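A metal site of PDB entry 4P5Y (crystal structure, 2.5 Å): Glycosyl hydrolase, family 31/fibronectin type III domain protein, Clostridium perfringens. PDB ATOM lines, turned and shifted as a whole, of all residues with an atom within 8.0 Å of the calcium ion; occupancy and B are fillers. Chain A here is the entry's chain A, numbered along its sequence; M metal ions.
O of Asn 42 is bound to the calcium ion. The backbone carbonyl oxygen (O) of Asp 47 binds the calcium ion (2.4 Å). OG1 of Thr 50 is bound to the calcium ion, 2.4 Å away. O of Ala 160 is bound to the calcium ion, at 2.4 Å. The calcium ion is bound by the side-chain carboxylate (OD1) of Asp 45, 2.5 Å away. The calcium ion is bound by O of Thr 50, at 2.6 Å.
The side-chain carboxylate of Asp 47 is in hydrogen-bond range of the backbone NH of Asn 49, at 3.0 Å. ND2 of Asn 42 sits close to N of Tyr 39 (3.3 Å). O of Ile 51 lies within hydrogen-bond range of ND2 of Asn 42 (3.0 Å). The backbone carbonyl oxygen of Leu 82 is in hydrogen-bond range of the backbone NH of Ala 160 (2.8 Å).
Five residues have an atom within 4 Å of the calcium ion: Asn 42, Asp 45, Asp 47, Thr 50 and Ala 160. The nearest printed residue that does not touch the calcium ion is Glu 161 (4.2 Å).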
ATOM      1  N   TYR A  39       8.060 -14.409 -23.869  1.00  0.00           N
ATOM      2  CA  TYR A  39       6.716 -14.807 -23.451  1.00  0.00           C
ATOM      3  C   TYR A  39       5.948 -13.738 -22.684  1.00  0.00           C
ATOM      4  O   TYR A  39       6.534 -12.877 -22.019  1.00  0.00           O
ATOM      5  CB  TYR A  39       6.783 -16.069 -22.580  1.00  0.00           C
ATOM      6  CG  TYR A  39       7.609 -17.160 -23.192  1.00  0.00           C
ATOM      7  CD1 TYR A  39       7.163 -17.837 -24.327  1.00  0.00           C
ATOM      8  CD2 TYR A  39       8.857 -17.494 -22.687  1.00  0.00           C
ATOM      9  CE1 TYR A  39       7.930 -18.839 -24.926  1.00  0.00           C
ATOM     10  CE2 TYR A  39       9.622 -18.488 -23.274  1.00  0.00           C
ATOM     11  CZ  TYR A  39       9.149 -19.155 -24.394  1.00  0.00           C
ATOM     12  OH  TYR A  39       9.901 -20.138 -24.999  1.00  0.00           O
ATOM     13  N   LYS A  40       4.632 -13.822 -22.755  1.00  0.00           N
ATOM     14  CA  LYS A  40       3.759 -12.882 -22.073  1.00  0.00           C
ATOM     15  C   LYS A  40       4.131 -12.747 -20.591  1.00  0.00           C
ATOM     16  O   LYS A  40       3.990 -11.685 -20.021  1.00  0.00           O
ATOM     17  CB  LYS A  40       2.301 -13.303 -22.240  1.00  0.00           C
ATOM     18  CG  LYS A  40       1.958 -14.668 -21.639  1.00  0.00           C
ATOM     19  CD  LYS A  40       0.501 -14.989 -21.830  1.00  0.00           C
ATOM     20  CE  LYS A  40       0.127 -16.383 -21.301  1.00  0.00           C
ATOM     21  NZ  LYS A  40       0.818 -17.494 -22.016  1.00  0.00           N
ATOM     22  N   GLU A  41       4.617 -13.826 -19.982  1.00  0.00           N
ATOM     23  CA  GLU A  41       4.990 -13.770 -18.560  1.00  0.00           C
ATOM     24  C   GLU A  41       6.143 -12.801 -18.293  1.00  0.00           C
ATOM     25  O   GLU A  41       6.370 -12.431 -17.153  1.00  0.00           O
ATOM     26  CB  GLU A  41       5.395 -15.168 -18.038  1.00  0.00           C
ATOM     27  CG  GLU A  41       4.277 -16.206 -18.012  1.00  0.00           C
ATOM     28  CD  GLU A  41       3.937 -16.737 -19.393  1.00  0.00           C
ATOM     29  OE1 GLU A  41       4.785 -16.584 -20.305  1.00  0.00           O
ATOM     30  OE2 GLU A  41       2.826 -17.309 -19.560  1.00  0.00           O
ATOM     31  N   ASN A  42       6.859 -12.408 -19.333  1.00  0.00           N
ATOM     32  CA  ASN A  42       8.016 -11.539 -19.114  1.00  0.00           C
ATOM     33  C   ASN A  42       7.627 -10.070 -18.964  1.00  0.00           C
ATOM     34  O   ASN A  42       8.459  -9.246 -18.605  1.00  0.00           O
ATOM     35  CB  ASN A  42       9.021 -11.698 -20.255  1.00  0.00           C
ATOM     36  CG  ASN A  42       9.671 -13.066 -20.293  1.00  0.00           C
ATOM     37  OD1 ASN A  42       9.776 -13.743 -19.274  1.00  0.00           O
ATOM     38  ND2 ASN A  42      10.103 -13.484 -21.469  1.00  0.00           N
ATOM     39  N   ALA A  43       6.375  -9.727 -19.245  1.00  0.00           N
ATOM     40  CA  ALA A  43       5.910  -8.366 -19.071  1.00  0.00           C
ATOM     41  C   ALA A  43       5.672  -7.993 -17.594  1.00  0.00           C
ATOM     42  O   ALA A  43       5.630  -6.815 -17.239  1.00  0.00           O
ATOM     43  CB  ALA A  43       4.639  -8.149 -19.852  1.00  0.00           C
ATOM     44  N   VAL A  44       5.514  -8.995 -16.740  1.00  0.00           N
ATOM     45  CA  VAL A  44       5.190  -8.733 -15.339  1.00  0.00           C
ATOM     46  C   VAL A  44       5.973  -9.593 -14.350  1.00  0.00           C
ATOM     47  O   VAL A  44       5.451  -9.985 -13.309  1.00  0.00           O
ATOM     48  CB  VAL A  44       3.706  -8.951 -15.082  1.00  0.00           C
ATOM     49  CG1 VAL A  44       2.892  -7.958 -15.906  1.00  0.00           C
ATOM     50  CG2 VAL A  44       3.318 -10.389 -15.405  1.00  0.00           C
ATOM     51  N   ASP A  45       7.230  -9.886 -14.675  1.00  0.00           N
ATOM     52  CA  ASP A  45       8.105 -10.680 -13.830  1.00  0.00           C
ATOM     53  C   ASP A  45       9.056  -9.812 -13.021  1.00  0.00           C
ATOM     54  O   ASP A  45      10.005 -10.308 -12.434  1.00  0.00           O
ATOM     55  CB  ASP A  45       8.898 -11.666 -14.682  1.00  0.00           C
ATOM     56  CG  ASP A  45       9.794 -10.994 -15.676  1.00  0.00           C
ATOM     57  OD1 ASP A  45       9.594  -9.783 -15.922  1.00  0.00           O
ATOM     58  OD2 ASP A  45      10.705 -11.658 -16.205  1.00  0.00           O
ATOM     59  N   GLY A  46       8.790  -8.509 -12.993  1.00  0.00           N
ATOM     60  CA  GLY A  46       9.640  -7.561 -12.297  1.00  0.00           C
ATOM     61  C   GLY A  46      11.074  -7.457 -12.802  1.00  0.00           C
ATOM     62  O   GLY A  46      11.967  -7.055 -12.074  1.00  0.00           O
ATOM     63  N   ASP A  47      11.301  -7.786 -14.067  1.00  0.00           N
ATOM     64  CA  ASP A  47      12.654  -7.899 -14.578  1.00  0.00           C
ATOM     65  C   ASP A  47      12.869  -7.100 -15.874  1.00  0.00           C
ATOM     66  O   ASP A  47      12.321  -7.428 -16.922  1.00  0.00           O
ATOM     67  CB  ASP A  47      12.958  -9.392 -14.803  1.00  0.00           C
ATOM     68  CG  ASP A  47      14.445  -9.662 -15.034  1.00  0.00           C
ATOM     69  OD1 ASP A  47      15.203  -8.717 -15.302  1.00  0.00           O
ATOM     70  OD2 ASP A  47      14.829 -10.848 -14.960  1.00  0.00           O
ATOM     71  N   GLU A  48      13.697  -6.058 -15.797  1.00  0.00           N
ATOM     72  CA  GLU A  48      14.033  -5.228 -16.958  1.00  0.00           C
ATOM     73  C   GLU A  48      14.662  -6.005 -18.124  1.00  0.00           C
ATOM     74  O   GLU A  48      14.668  -5.531 -19.254  1.00  0.00           O
ATOM     75  CB  GLU A  48      15.012  -4.102 -16.573  1.00  0.00           C
ATOM     76  CG  GLU A  48      15.123  -3.800 -15.084  1.00  0.00           C
ATOM     77  CD  GLU A  48      15.979  -4.807 -14.318  1.00  0.00           C
ATOM     78  OE1 GLU A  48      17.224  -4.791 -14.477  1.00  0.00           O
ATOM     79  OE2 GLU A  48      15.388  -5.605 -13.560  1.00  0.00           O
ATOM     80  N   ASN A  49      15.215  -7.170 -17.825  1.00  0.00           N
ATOM     81  CA  ASN A  49      16.035  -7.872 -18.810  1.00  0.00           C
ATOM     82  C   ASN A  49      15.273  -8.955 -19.553  1.00  0.00           C
ATOM     83  O   ASN A  49      15.823  -9.656 -20.389  1.00  0.00           O
ATOM     84  CB  ASN A  49      17.288  -8.453 -18.137  1.00  0.00           C
ATOM     85  CG  ASN A  49      18.320  -7.391 -17.821  1.00  0.00           C
ATOM     86  OD1 ASN A  49      18.619  -6.548 -18.657  1.00  0.00           O
ATOM     87  ND2 ASN A  49      18.849  -7.402 -16.589  1.00  0.00           N
ATOM     88  N   THR A  50      14.001  -9.104 -19.233  1.00  0.00           N
ATOM     89  CA  THR A  50      13.136  -9.976 -19.999  1.00  0.00           C
ATOM     90  C   THR A  50      12.044  -9.156 -20.683  1.00  0.00           C
ATOM     91  O   THR A  50      11.590  -8.132 -20.156  1.00  0.00           O
ATOM     92  CB  THR A  50      12.487 -11.071 -19.122  1.00  0.00           C
ATOM     93  OG1 THR A  50      11.627 -10.463 -18.148  1.00  0.00           O
ATOM     94  CG2 THR A  50      13.558 -11.888 -18.403  1.00  0.00           C
ATOM     95  N   ILE A  51      11.637  -9.589 -21.861  1.00  0.00           N
ATOM     96  CA  ILE A  51      10.526  -8.923 -22.525  1.00  0.00           C
ATOM     97  C   ILE A  51       9.467  -9.899 -23.010  1.00  0.00           C
ATOM     98  O   ILE A  51       9.723 -11.078 -23.236  1.00  0.00           O
ATOM     99  CB  ILE A  51      10.996  -8.097 -23.742  1.00  0.00           C
ATOM    100  CG1 ILE A  51      11.416  -9.028 -24.881  1.00  0.00           C
ATOM    101  CG2 ILE A  51      12.109  -7.132 -23.322  1.00  0.00           C
ATOM    102  CD1 ILE A  51      12.023  -8.312 -26.059  1.00  0.00           C
ATOM    103  N   TRP A  52       8.257  -9.374 -23.141  1.00  0.00           N
ATOM    104  CA  TRP A  52       7.268  -9.948 -24.035  1.00  0.00           C
ATOM    105  C   TRP A  52       7.413  -9.308 -25.410  1.00  0.00           C
ATOM    106  O   TRP A  52       7.510  -8.097 -25.528  1.00  0.00           O
ATOM    107  CB  TRP A  52       5.863  -9.722 -23.508  1.00  0.00           C
ATOM    108  CG  TRP A  52       4.813  -9.993 -24.522  1.00  0.00           C
ATOM    109  CD1 TRP A  52       4.563 -11.179 -25.147  1.00  0.00           C
ATOM    110  CD2 TRP A  52       3.842  -9.068 -25.021  1.00  0.00           C
ATOM    111  NE1 TRP A  52       3.497 -11.055 -26.003  1.00  0.00           N
ATOM    112  CE2 TRP A  52       3.037  -9.766 -25.952  1.00  0.00           C
ATOM    113  CE3 TRP A  52       3.557  -7.722 -24.765  1.00  0.00           C
ATOM    114  CZ2 TRP A  52       1.985  -9.154 -26.632  1.00  0.00           C
ATOM    115  CZ3 TRP A  52       2.507  -7.117 -25.458  1.00  0.00           C
ATOM    116  CH2 TRP A  52       1.735  -7.837 -26.370  1.00  0.00           C
ATOM    117  N   LEU A  82       7.606  -0.097 -19.226  1.00  0.00           N
ATOM    118  CA  LEU A  82       9.050  -0.108 -19.383  1.00  0.00           C
ATOM    119  C   LEU A  82       9.465  -0.690 -20.715  1.00  0.00           C
ATOM    120  O   LEU A  82       9.338  -1.898 -20.943  1.00  0.00           O
ATOM    121  CB  LEU A  82       9.712  -0.902 -18.271  1.00  0.00           C
ATOM    122  CG  LEU A  82      11.232  -0.883 -18.324  1.00  0.00           C
ATOM    123  CD1 LEU A  82      11.786   0.534 -18.133  1.00  0.00           C
ATOM    124  CD2 LEU A  82      11.765  -1.817 -17.270  1.00  0.00           C
ATOM    125  N   ALA A 159       7.200  -5.354 -24.487  1.00  0.00           N
ATOM    126  CA  ALA A 159       7.214  -4.649 -23.214  1.00  0.00           C
ATOM    127  C   ALA A 159       8.171  -5.376 -22.287  1.00  0.00           C
ATOM    128  O   ALA A 159       8.125  -6.606 -22.173  1.00  0.00           O
ATOM    129  CB  ALA A 159       5.814  -4.573 -22.600  1.00  0.00           C
ATOM    130  N   ALA A 160       9.029  -4.607 -21.643  1.00  0.00           N
ATOM    131  CA  ALA A 160       9.958  -5.173 -20.672  1.00  0.00           C
ATOM    132  C   ALA A 160       9.240  -5.353 -19.343  1.00  0.00           C
ATOM    133  O   ALA A 160       9.367  -6.385 -18.702  1.00  0.00           O
ATOM    134  CB  ALA A 160      11.210  -4.287 -20.513  1.00  0.00           C
ATOM    135  N   GLU A 161       8.457  -4.351 -18.945  1.00  0.00           N
ATOM    136  CA  GLU A 161       7.691  -4.433 -17.706  1.00  0.00           C
ATOM    137  C   GLU A 161       6.391  -3.672 -17.765  1.00  0.00           C
ATOM    138  O   GLU A 161       6.275  -2.631 -18.426  1.00  0.00           O
ATOM    139  CB  GLU A 161       8.486  -3.899 -16.526  1.00  0.00           C
ATOM    140  CG  GLU A 161       9.501  -4.821 -15.913  1.00  0.00           C
ATOM    141  CD  GLU A 161       9.868  -4.385 -14.488  1.00  0.00           C
ATOM    142  OE1 GLU A 161      10.831  -3.596 -14.308  1.00  0.00           O
ATOM    143  OE2 GLU A 161       9.176  -4.811 -13.541  1.00  0.00           O
ATOM    144  N   LEU A 162       5.407  -4.184 -17.043  1.00  0.00           N
ATOM    145  CA  LEU A 162       4.253  -3.396 -16.654  1.00  0.00           C
ATOM    146  C   LEU A 162       4.212  -3.366 -15.135  1.00  0.00           C
ATOM    147  O   LEU A 162       4.095  -4.415 -14.486  1.00  0.00           O
ATOM    148  CB  LEU A 162       2.958  -3.972 -17.215  1.00  0.00           C
ATOM    149  CG  LEU A 162       2.936  -4.049 -18.726  1.00  0.00           C
ATOM    150  CD1 LEU A 162       1.735  -4.844 -19.185  1.00  0.00           C
ATOM    151  CD2 LEU A 162       2.920  -2.629 -19.307  1.00  0.00           C
HETATM  152 CA    CA M   1      10.401  -8.416 -17.877  1.00  0.00          CA
